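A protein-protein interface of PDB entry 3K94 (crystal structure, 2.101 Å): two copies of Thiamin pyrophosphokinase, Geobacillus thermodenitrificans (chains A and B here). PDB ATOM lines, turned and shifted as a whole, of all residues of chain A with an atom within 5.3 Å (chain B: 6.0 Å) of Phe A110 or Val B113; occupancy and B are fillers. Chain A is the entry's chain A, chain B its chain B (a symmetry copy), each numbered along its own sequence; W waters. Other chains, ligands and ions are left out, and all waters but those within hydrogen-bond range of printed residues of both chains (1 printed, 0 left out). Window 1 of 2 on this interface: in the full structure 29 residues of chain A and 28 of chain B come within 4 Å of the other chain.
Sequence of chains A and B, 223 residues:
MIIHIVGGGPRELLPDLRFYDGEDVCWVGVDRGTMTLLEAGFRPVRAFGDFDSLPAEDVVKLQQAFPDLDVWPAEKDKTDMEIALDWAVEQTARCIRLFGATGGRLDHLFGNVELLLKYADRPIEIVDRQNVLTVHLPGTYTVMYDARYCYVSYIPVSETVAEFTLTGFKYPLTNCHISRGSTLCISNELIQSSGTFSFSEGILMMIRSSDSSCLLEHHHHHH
Leu B109 touches its own counterpart, Leu A109.
Leu A109 touches Phe B110, and with the chains exchanged Phe A110 touches Leu B109.
Phe B110 touches its own counterpart, Phe A110.
Phe A110 touches Val B113, and with the chains exchanged Val A113 touches Phe B110.
Of the 16 pairs that touch across the chains among the printed residues, 6 have their exchanged pair printed and touching as well.
Among the printed residues, merely in contact across the chains: Leu A106 with Leu B109 (3.9 Å), Leu A106 with Ile B207 (3.9 Å), Asp A107 with Ile B207 (3.9 Å), Leu A109 with Leu B109 (3.7 Å), Leu A109 with Phe B110 (3.998 Å), Phe A110 with Leu B109 (3.8 Å), Phe A110 with Phe B110 (3.4 Å), Phe A110 with Val B113 (3.7 Å), Phe A110 with Leu B133 (3.6 Å), Phe A110 with Ile B155 (3.6 Å), Phe A110 with Met B205 (3.9 Å), Phe A110 with Ile B207 (3.7 Å), Gly A111 with Ile B155 (3.9 Å), Val A113 with Phe B110 (3.9 Å), Glu A114 with Ile B155 (3.8 Å) and Glu A114 with Leu B184 (3.4 Å).
Water W1 lies within hydrogen-bond range of the backbone carbonyl oxygen (O) of Ile B207 (2.8 Å) and the side-chain carboxylate (OD2) of Asp A107 (3.4 Å).
The backbone carbonyl oxygen of Ile B126 is in hydrogen-bond range of the backbone NH of Leu B133 (2.8 Å).
N of Met B205 is in hydrogen-bond range of O of Ile B155 (2.7 Å).
Phe A110 touches seven residues of chain B.
Of the printed residues of chain A, Val B113 touches Phe A110 (3.7 Å).
Of the printed residues of chain B, Val A113 touches Phe B110.
Of the printed residues of chain A, Leu B133 touches Phe A110.
Of the printed residues of chain B, Leu A109 touches Leu B109 (3.7 Å) and Phe B110 (3.998 Å).
Of the printed residues of chain A, Phe B110 touches Leu A109 (3.998 Å), Phe A110 (3.4 Å) and Val A113 (3.9 Å).
Of the printed residues of chain A, Leu B184 touches Glu A114.
Asn B112 touches none of the printed residues of chain A.
The nearest printed residue of chain A that does not touch Val B113 is Leu A106 (7.3 Å).
Of the 18 printed residues of chain B, 8 touch a printed residue of chain A.
Hydrophobic or aromatic side chains of chain B within 4 Å of the printed part of chain A: Leu B109, Phe B110, Val B113, Leu B133, Ile B155, Leu B184, Met B205 and Ile B207.
Hydrophobic or aromatic side chains of chain A within 4 Å of the printed part of chain B: Leu A106, Leu A109, Phe A110 and Val A113.
Among the printed residues, 16 pairs touch across the chains.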
ATOM      1  N   LEU A 106       9.072 -23.731  16.995  1.00  0.00           N
ATOM      2  CA  LEU A 106       8.695 -22.442  17.555  1.00  0.00           C
ATOM      3  C   LEU A 106       9.024 -21.283  16.625  1.00  0.00           C
ATOM      4  O   LEU A 106       8.464 -20.199  16.773  1.00  0.00           O
ATOM      5  CB  LEU A 106       9.360 -22.237  18.911  1.00  0.00           C
ATOM      6  CG  LEU A 106       8.899 -23.220  19.994  1.00  0.00           C
ATOM      7  CD1 LEU A 106       9.828 -23.140  21.193  1.00  0.00           C
ATOM      8  CD2 LEU A 106       7.452 -22.968  20.378  1.00  0.00           C
ATOM      9  N   ASP A 107       9.923 -21.500  15.666  1.00  0.00           N
ATOM     10  CA  ASP A 107      10.180 -20.454  14.671  1.00  0.00           C
ATOM     11  C   ASP A 107       8.917 -20.197  13.851  1.00  0.00           C
ATOM     12  O   ASP A 107       8.683 -19.085  13.398  1.00  0.00           O
ATOM     13  CB  ASP A 107      11.365 -20.797  13.776  1.00  0.00           C
ATOM     14  CG  ASP A 107      11.266 -22.193  13.202  1.00  0.00           C
ATOM     15  OD1 ASP A 107      11.124 -23.162  13.980  1.00  0.00           O
ATOM     16  OD2 ASP A 107      11.319 -22.321  11.968  1.00  0.00           O
ATOM     17  N   HIS A 108       8.082 -21.215  13.697  1.00  0.00           N
ATOM     18  CA  HIS A 108       6.796 -20.999  13.034  1.00  0.00           C
ATOM     19  C   HIS A 108       5.905 -20.084  13.866  1.00  0.00           C
ATOM     20  O   HIS A 108       5.396 -19.080  13.358  1.00  0.00           O
ATOM     21  CB  HIS A 108       6.086 -22.317  12.723  1.00  0.00           C
ATOM     22  CG  HIS A 108       6.689 -23.060  11.573  1.00  0.00           C
ATOM     23  ND1 HIS A 108       6.491 -24.409  11.367  1.00  0.00           N
ATOM     24  CD2 HIS A 108       7.492 -22.639  10.565  1.00  0.00           C
ATOM     25  CE1 HIS A 108       7.140 -24.785  10.277  1.00  0.00           C
ATOM     26  NE2 HIS A 108       7.759 -23.731   9.775  1.00  0.00           N
ATOM     27  N   LEU A 109       5.721 -20.432  15.141  1.00  0.00           N
ATOM     28  CA  LEU A 109       4.910 -19.614  16.036  1.00  0.00           C
ATOM     29  C   LEU A 109       5.384 -18.164  16.078  1.00  0.00           C
ATOM     30  O   LEU A 109       4.598 -17.242  15.885  1.00  0.00           O
ATOM     31  CB  LEU A 109       4.896 -20.193  17.456  1.00  0.00           C
ATOM     32  CG  LEU A 109       4.236 -19.268  18.481  1.00  0.00           C
ATOM     33  CD1 LEU A 109       2.758 -19.154  18.213  1.00  0.00           C
ATOM     34  CD2 LEU A 109       4.480 -19.745  19.914  1.00  0.00           C
ATOM     35  N   PHE A 110       6.671 -17.964  16.347  1.00  0.00           N
ATOM     36  CA  PHE A 110       7.197 -16.612  16.509  1.00  0.00           C
ATOM     37  C   PHE A 110       7.128 -15.812  15.210  1.00  0.00           C
ATOM     38  O   PHE A 110       6.797 -14.631  15.230  1.00  0.00           O
ATOM     39  CB  PHE A 110       8.595 -16.636  17.148  1.00  0.00           C
ATOM     40  CG  PHE A 110       8.553 -16.929  18.630  1.00  0.00           C
ATOM     41  CD1 PHE A 110       8.303 -15.917  19.539  1.00  0.00           C
ATOM     42  CD2 PHE A 110       8.699 -18.223  19.101  1.00  0.00           C
ATOM     43  CE1 PHE A 110       8.227 -16.182  20.893  1.00  0.00           C
ATOM     44  CE2 PHE A 110       8.627 -18.500  20.457  1.00  0.00           C
ATOM     45  CZ  PHE A 110       8.386 -17.480  21.356  1.00  0.00           C
ATOM     46  N   GLY A 111       7.392 -16.469  14.085  1.00  0.00           N
ATOM     47  CA  GLY A 111       7.221 -15.843  12.783  1.00  0.00           C
ATOM     48  C   GLY A 111       5.768 -15.468  12.529  1.00  0.00           C
ATOM     49  O   GLY A 111       5.490 -14.404  11.984  1.00  0.00           O
ATOM     50  N   ASN A 112       4.843 -16.338  12.928  1.00  0.00           N
ATOM     51  CA  ASN A 112       3.413 -16.028  12.815  1.00  0.00           C
ATOM     52  C   ASN A 112       2.993 -14.832  13.667  1.00  0.00           C
ATOM     53  O   ASN A 112       2.146 -14.029  13.257  1.00  0.00           O
ATOM     54  CB  ASN A 112       2.560 -17.255  13.135  1.00  0.00           C
ATOM     55  CG  ASN A 112       2.644 -18.302  12.045  1.00  0.00           C
ATOM     56  OD1 ASN A 112       2.899 -17.969  10.904  1.00  0.00           O
ATOM     57  ND2 ASN A 112       2.446 -19.561  12.393  1.00  0.00           N
ATOM     58  N   VAL A 113       3.597 -14.701  14.846  1.00  0.00           N
ATOM     59  CA  VAL A 113       3.332 -13.539  15.691  1.00  0.00           C
ATOM     60  C   VAL A 113       3.832 -12.250  15.015  1.00  0.00           C
ATOM     61  O   VAL A 113       3.156 -11.229  15.070  1.00  0.00           O
ATOM     62  CB  VAL A 113       3.883 -13.699  17.138  1.00  0.00           C
ATOM     63  CG1 VAL A 113       3.800 -12.368  17.893  1.00  0.00           C
ATOM     64  CG2 VAL A 113       3.093 -14.791  17.907  1.00  0.00           C
ATOM     65  N   GLU A 114       4.986 -12.308  14.349  1.00  0.00           N
ATOM     66  CA  GLU A 114       5.474 -11.154  13.586  1.00  0.00           C
ATOM     67  C   GLU A 114       4.503 -10.764  12.461  1.00  0.00           C
ATOM     68  O   GLU A 114       4.351  -9.573  12.157  1.00  0.00           O
ATOM     69  CB  GLU A 114       6.891 -11.385  13.022  1.00  0.00           C
ATOM     70  CG  GLU A 114       7.990 -11.619  14.091  1.00  0.00           C
ATOM     71  CD  GLU A 114       8.197 -10.434  15.043  1.00  0.00           C
ATOM     72  OE1 GLU A 114       8.436  -9.308  14.571  1.00  0.00           O
ATOM     73  OE2 GLU A 114       8.125 -10.627  16.278  1.00  0.00           O
ATOM     74  N   HIS B 108       2.632 -18.612  29.153  1.00  0.00           N
ATOM     75  CA  HIS B 108       3.806 -19.158  29.852  1.00  0.00           C
ATOM     76  C   HIS B 108       5.083 -19.080  29.010  1.00  0.00           C
ATOM     77  O   HIS B 108       6.121 -18.593  29.478  1.00  0.00           O
ATOM     78  CB  HIS B 108       3.554 -20.596  30.327  1.00  0.00           C
ATOM     79  CG  HIS B 108       2.508 -20.700  31.395  1.00  0.00           C
ATOM     80  ND1 HIS B 108       1.893 -21.891  31.728  1.00  0.00           N
ATOM     81  CD2 HIS B 108       1.955 -19.755  32.194  1.00  0.00           C
ATOM     82  CE1 HIS B 108       1.009 -21.674  32.687  1.00  0.00           C
ATOM     83  NE2 HIS B 108       1.026 -20.386  32.986  1.00  0.00           N
ATOM     84  N   LEU B 109       5.010 -19.550  27.768  1.00  0.00           N
ATOM     85  CA  LEU B 109       6.159 -19.455  26.869  1.00  0.00           C
ATOM     86  C   LEU B 109       6.584 -17.999  26.658  1.00  0.00           C
ATOM     87  O   LEU B 109       7.766 -17.661  26.683  1.00  0.00           O
ATOM     88  CB  LEU B 109       5.864 -20.107  25.517  1.00  0.00           C
ATOM     89  CG  LEU B 109       6.896 -19.779  24.427  1.00  0.00           C
ATOM     90  CD1 LEU B 109       8.262 -20.351  24.738  1.00  0.00           C
ATOM     91  CD2 LEU B 109       6.428 -20.260  23.056  1.00  0.00           C
ATOM     92  N   PHE B 110       5.616 -17.130  26.459  1.00  0.00           N
ATOM     93  CA  PHE B 110       5.952 -15.747  26.127  1.00  0.00           C
ATOM     94  C   PHE B 110       6.511 -15.022  27.332  1.00  0.00           C
ATOM     95  O   PHE B 110       7.420 -14.219  27.201  1.00  0.00           O
ATOM     96  CB  PHE B 110       4.757 -15.022  25.500  1.00  0.00           C
ATOM     97  CG  PHE B 110       4.570 -15.362  24.046  1.00  0.00           C
ATOM     98  CD1 PHE B 110       5.315 -14.720  23.075  1.00  0.00           C
ATOM     99  CD2 PHE B 110       3.694 -16.353  23.661  1.00  0.00           C
ATOM    100  CE1 PHE B 110       5.159 -15.042  21.748  1.00  0.00           C
ATOM    101  CE2 PHE B 110       3.537 -16.681  22.331  1.00  0.00           C
ATOM    102  CZ  PHE B 110       4.267 -16.030  21.376  1.00  0.00           C
ATOM    103  N   GLY B 111       5.979 -15.339  28.507  1.00  0.00           N
ATOM    104  CA  GLY B 111       6.522 -14.812  29.744  1.00  0.00           C
ATOM    105  C   GLY B 111       7.949 -15.276  29.927  1.00  0.00           C
ATOM    106  O   GLY B 111       8.819 -14.492  30.288  1.00  0.00           O
ATOM    107  N   ASN B 112       8.191 -16.558  29.659  1.00  0.00           N
ATOM    108  CA  ASN B 112       9.540 -17.104  29.710  1.00  0.00           C
ATOM    109  C   ASN B 112      10.521 -16.441  28.746  1.00  0.00           C
ATOM    110  O   ASN B 112      11.673 -16.219  29.108  1.00  0.00           O
ATOM    111  CB  ASN B 112       9.507 -18.619  29.524  1.00  0.00           C
ATOM    112  CG  ASN B 112       8.957 -19.310  30.745  1.00  0.00           C
ATOM    113  OD1 ASN B 112       9.095 -18.787  31.845  1.00  0.00           O
ATOM    114  ND2 ASN B 112       8.337 -20.473  30.572  1.00  0.00           N
ATOM    115  N   VAL B 113      10.065 -16.116  27.534  1.00  0.00           N
ATOM    116  CA  VAL B 113      10.895 -15.383  26.570  1.00  0.00           C
ATOM    117  C   VAL B 113      11.227 -13.974  27.098  1.00  0.00           C
ATOM    118  O   VAL B 113      12.342 -13.485  26.918  1.00  0.00           O
ATOM    119  CB  VAL B 113      10.222 -15.279  25.174  1.00  0.00           C
ATOM    120  CG1 VAL B 113      10.994 -14.340  24.276  1.00  0.00           C
ATOM    121  CG2 VAL B 113      10.124 -16.654  24.508  1.00  0.00           C
ATOM    122  N   GLU B 114      10.264 -13.329  27.759  1.00  0.00           N
ATOM    123  CA  GLU B 114      10.522 -12.027  28.381  1.00  0.00           C
ATOM    124  C   GLU B 114      11.615 -12.110  29.459  1.00  0.00           C
ATOM    125  O   GLU B 114      12.390 -11.168  29.638  1.00  0.00           O
ATOM    126  CB  GLU B 114       9.233 -11.412  28.941  1.00  0.00           C
ATOM    127  CG  GLU B 114       8.198 -11.086  27.850  1.00  0.00           C
ATOM    128  CD  GLU B 114       8.726 -10.101  26.810  1.00  0.00           C
ATOM    129  OE1 GLU B 114       9.288  -9.055  27.202  1.00  0.00           O
ATOM    130  OE2 GLU B 114       8.567 -10.364  25.596  1.00  0.00           O
ATOM    131  N   LEU B 115      11.676 -13.236  30.167  1.00  0.00           N
ATOM    132  CA  LEU B 115      12.760 -13.489  31.124  1.00  0.00           C
ATOM    133  C   LEU B 115      14.114 -13.566  30.422  1.00  0.00           C
ATOM    134  O   LEU B 115      15.091 -12.975  30.875  1.00  0.00           O
ATOM    135  CB  LEU B 115      12.516 -14.787  31.899  1.00  0.00           C
ATOM    136  CG  LEU B 115      11.503 -14.739  33.037  1.00  0.00           C
ATOM    137  CD1 LEU B 115      11.141 -16.144  33.483  1.00  0.00           C
ATOM    138  CD2 LEU B 115      12.098 -13.957  34.188  1.00  0.00           C
ATOM    139  N   LEU B 116      14.181 -14.295  29.312  1.00  0.00           N
ATOM    140  CA  LEU B 116      15.415 -14.313  28.540  1.00  0.00           C
ATOM    141  C   LEU B 116      15.831 -12.892  28.124  1.00  0.00           C
ATOM    142  O   LEU B 116      17.015 -12.529  28.182  1.00  0.00           O
ATOM    143  CB  LEU B 116      15.291 -15.242  27.331  1.00  0.00           C
ATOM    144  CG  LEU B 116      15.711 -16.694  27.600  1.00  0.00           C
ATOM    145  CD1 LEU B 116      14.962 -17.256  28.787  1.00  0.00           C
ATOM    146  CD2 LEU B 116      15.504 -17.563  26.359  1.00  0.00           C
ATOM    147  N   LEU B 117      14.854 -12.092  27.709  1.00  0.00           N
ATOM    148  CA  LEU B 117      15.112 -10.706  27.321  1.00  0.00           C
ATOM    149  C   LEU B 117      15.594  -9.860  28.478  1.00  0.00           C
ATOM    150  O   LEU B 117      16.525  -9.076  28.329  1.00  0.00           O
ATOM    151  CB  LEU B 117      13.865 -10.068  26.724  1.00  0.00           C
ATOM    152  CG  LEU B 117      13.526 -10.692  25.383  1.00  0.00           C
ATOM    153  CD1 LEU B 117      12.164 -10.214  24.932  1.00  0.00           C
ATOM    154  CD2 LEU B 117      14.629 -10.348  24.381  1.00  0.00           C
ATOM    155  N   LYS B 118      14.955 -10.012  29.632  1.00  0.00           N
ATOM    156  CA  LYS B 118      15.402  -9.305  30.821  1.00  0.00           C
ATOM    157  C   LYS B 118      16.862  -9.628  31.109  1.00  0.00           C
ATOM    158  O   LYS B 118      17.637  -8.745  31.479  1.00  0.00           O
ATOM    159  CB  LYS B 118      14.531  -9.636  32.030  1.00  0.00           C
ATOM    160  CG  LYS B 118      15.099  -9.095  33.339  1.00  0.00           C
ATOM    161  CD  LYS B 118      14.172  -9.368  34.507  1.00  0.00           C
ATOM    162  CE  LYS B 118      14.718  -8.789  35.802  1.00  0.00           C
ATOM    163  NZ  LYS B 118      13.688  -8.857  36.873  1.00  0.00           N
ATOM    164  N   ILE B 126      16.203 -21.598  26.064  1.00  0.00           N
ATOM    165  CA  ILE B 126      15.006 -22.399  26.258  1.00  0.00           C
ATOM    166  C   ILE B 126      15.113 -23.616  25.342  1.00  0.00           C
ATOM    167  O   ILE B 126      15.383 -23.487  24.133  1.00  0.00           O
ATOM    168  CB  ILE B 126      13.734 -21.589  25.929  1.00  0.00           C
ATOM    169  CG1 ILE B 126      13.498 -20.526  27.008  1.00  0.00           C
ATOM    170  CG2 ILE B 126      12.533 -22.515  25.792  1.00  0.00           C
ATOM    171  CD1 ILE B 126      12.336 -19.574  26.708  1.00  0.00           C
ATOM    172  N   LEU B 133      15.900 -21.961  21.874  1.00  0.00           N
ATOM    173  CA  LEU B 133      15.597 -20.558  21.643  1.00  0.00           C
ATOM    174  C   LEU B 133      16.499 -19.716  22.522  1.00  0.00           C
ATOM    175  O   LEU B 133      16.700 -20.030  23.697  1.00  0.00           O
ATOM    176  CB  LEU B 133      14.103 -20.279  21.904  1.00  0.00           C
ATOM    177  CG  LEU B 133      13.538 -18.868  21.690  1.00  0.00           C
ATOM    178  CD1 LEU B 133      12.032 -18.934  21.535  1.00  0.00           C
ATOM    179  CD2 LEU B 133      13.910 -17.945  22.858  1.00  0.00           C
ATOM    180  N   VAL B 135      18.148 -15.391  22.956  1.00  0.00           N
ATOM    181  CA  VAL B 135      18.106 -13.984  22.561  1.00  0.00           C
ATOM    182  C   VAL B 135      19.488 -13.377  22.785  1.00  0.00           C
ATOM    183  O   VAL B 135      20.227 -13.818  23.668  1.00  0.00           O
ATOM    184  CB  VAL B 135      17.019 -13.191  23.332  1.00  0.00           C
ATOM    185  CG1 VAL B 135      15.634 -13.825  23.114  1.00  0.00           C
ATOM    186  CG2 VAL B 135      17.354 -13.141  24.799  1.00  0.00           C
ATOM    187  N   ILE B 155      14.950 -13.635  14.316  1.00  0.00           N
ATOM    188  CA  ILE B 155      13.865 -12.681  14.443  1.00  0.00           C
ATOM    189  C   ILE B 155      14.319 -11.482  15.259  1.00  0.00           C
ATOM    190  O   ILE B 155      14.804 -11.644  16.375  1.00  0.00           O
ATOM    191  CB  ILE B 155      12.641 -13.317  15.104  1.00  0.00           C
ATOM    192  CG1 ILE B 155      12.131 -14.465  14.244  1.00  0.00           C
ATOM    193  CG2 ILE B 155      11.534 -12.280  15.302  1.00  0.00           C
ATOM    194  CD1 ILE B 155      10.975 -15.225  14.856  1.00  0.00           C
ATOM    195  N   LEU B 184      10.343 -10.093   8.848  1.00  0.00           N
ATOM    196  CA  LEU B 184       9.577 -10.810   9.859  1.00  0.00           C
ATOM    197  C   LEU B 184      10.422 -11.866  10.541  1.00  0.00           C
ATOM    198  O   LEU B 184      10.392 -12.016  11.758  1.00  0.00           O
ATOM    199  CB  LEU B 184       8.351 -11.465   9.224  1.00  0.00           C
ATOM    200  CG  LEU B 184       7.451 -10.488   8.464  1.00  0.00           C
ATOM    201  CD1 LEU B 184       6.397 -11.230   7.657  1.00  0.00           C
ATOM    202  CD2 LEU B 184       6.810  -9.481   9.404  1.00  0.00           C
ATOM    203  N   MET B 205      16.614 -12.479  18.218  1.00  0.00           N
ATOM    204  CA  MET B 205      16.261 -13.815  18.659  1.00  0.00           C
ATOM    205  C   MET B 205      16.713 -14.861  17.658  1.00  0.00           C
ATOM    206  O   MET B 205      16.492 -14.712  16.460  1.00  0.00           O
ATOM    207  CB  MET B 205      14.748 -13.920  18.873  1.00  0.00           C
ATOM    208  CG  MET B 205      14.290 -15.315  19.243  1.00  0.00           C
ATOM    209  SD  MET B 205      12.356 -15.453  19.611  1.00  0.00           S
ATOM    210  CE  MET B 205      11.667 -14.489  18.071  1.00  0.00           C
ATOM    211  N   ILE B 207      16.229 -18.979  16.774  1.00  0.00           N
ATOM    212  CA  ILE B 207      15.647 -20.281  17.046  1.00  0.00           C
ATOM    213  C   ILE B 207      16.247 -21.330  16.116  1.00  0.00           C
ATOM    214  O   ILE B 207      16.227 -21.171  14.900  1.00  0.00           O
ATOM    215  CB  ILE B 207      14.116 -20.263  16.914  1.00  0.00           C
ATOM    216  CG1 ILE B 207      13.509 -19.314  17.953  1.00  0.00           C
ATOM    217  CG2 ILE B 207      13.562 -21.680  17.092  1.00  0.00           C
ATOM    218  CD1 ILE B 207      12.058 -18.906  17.658  1.00  0.00           C
HETATM  219  O   HOH W   1      14.428 -22.552  13.269  1.00  0.00           O
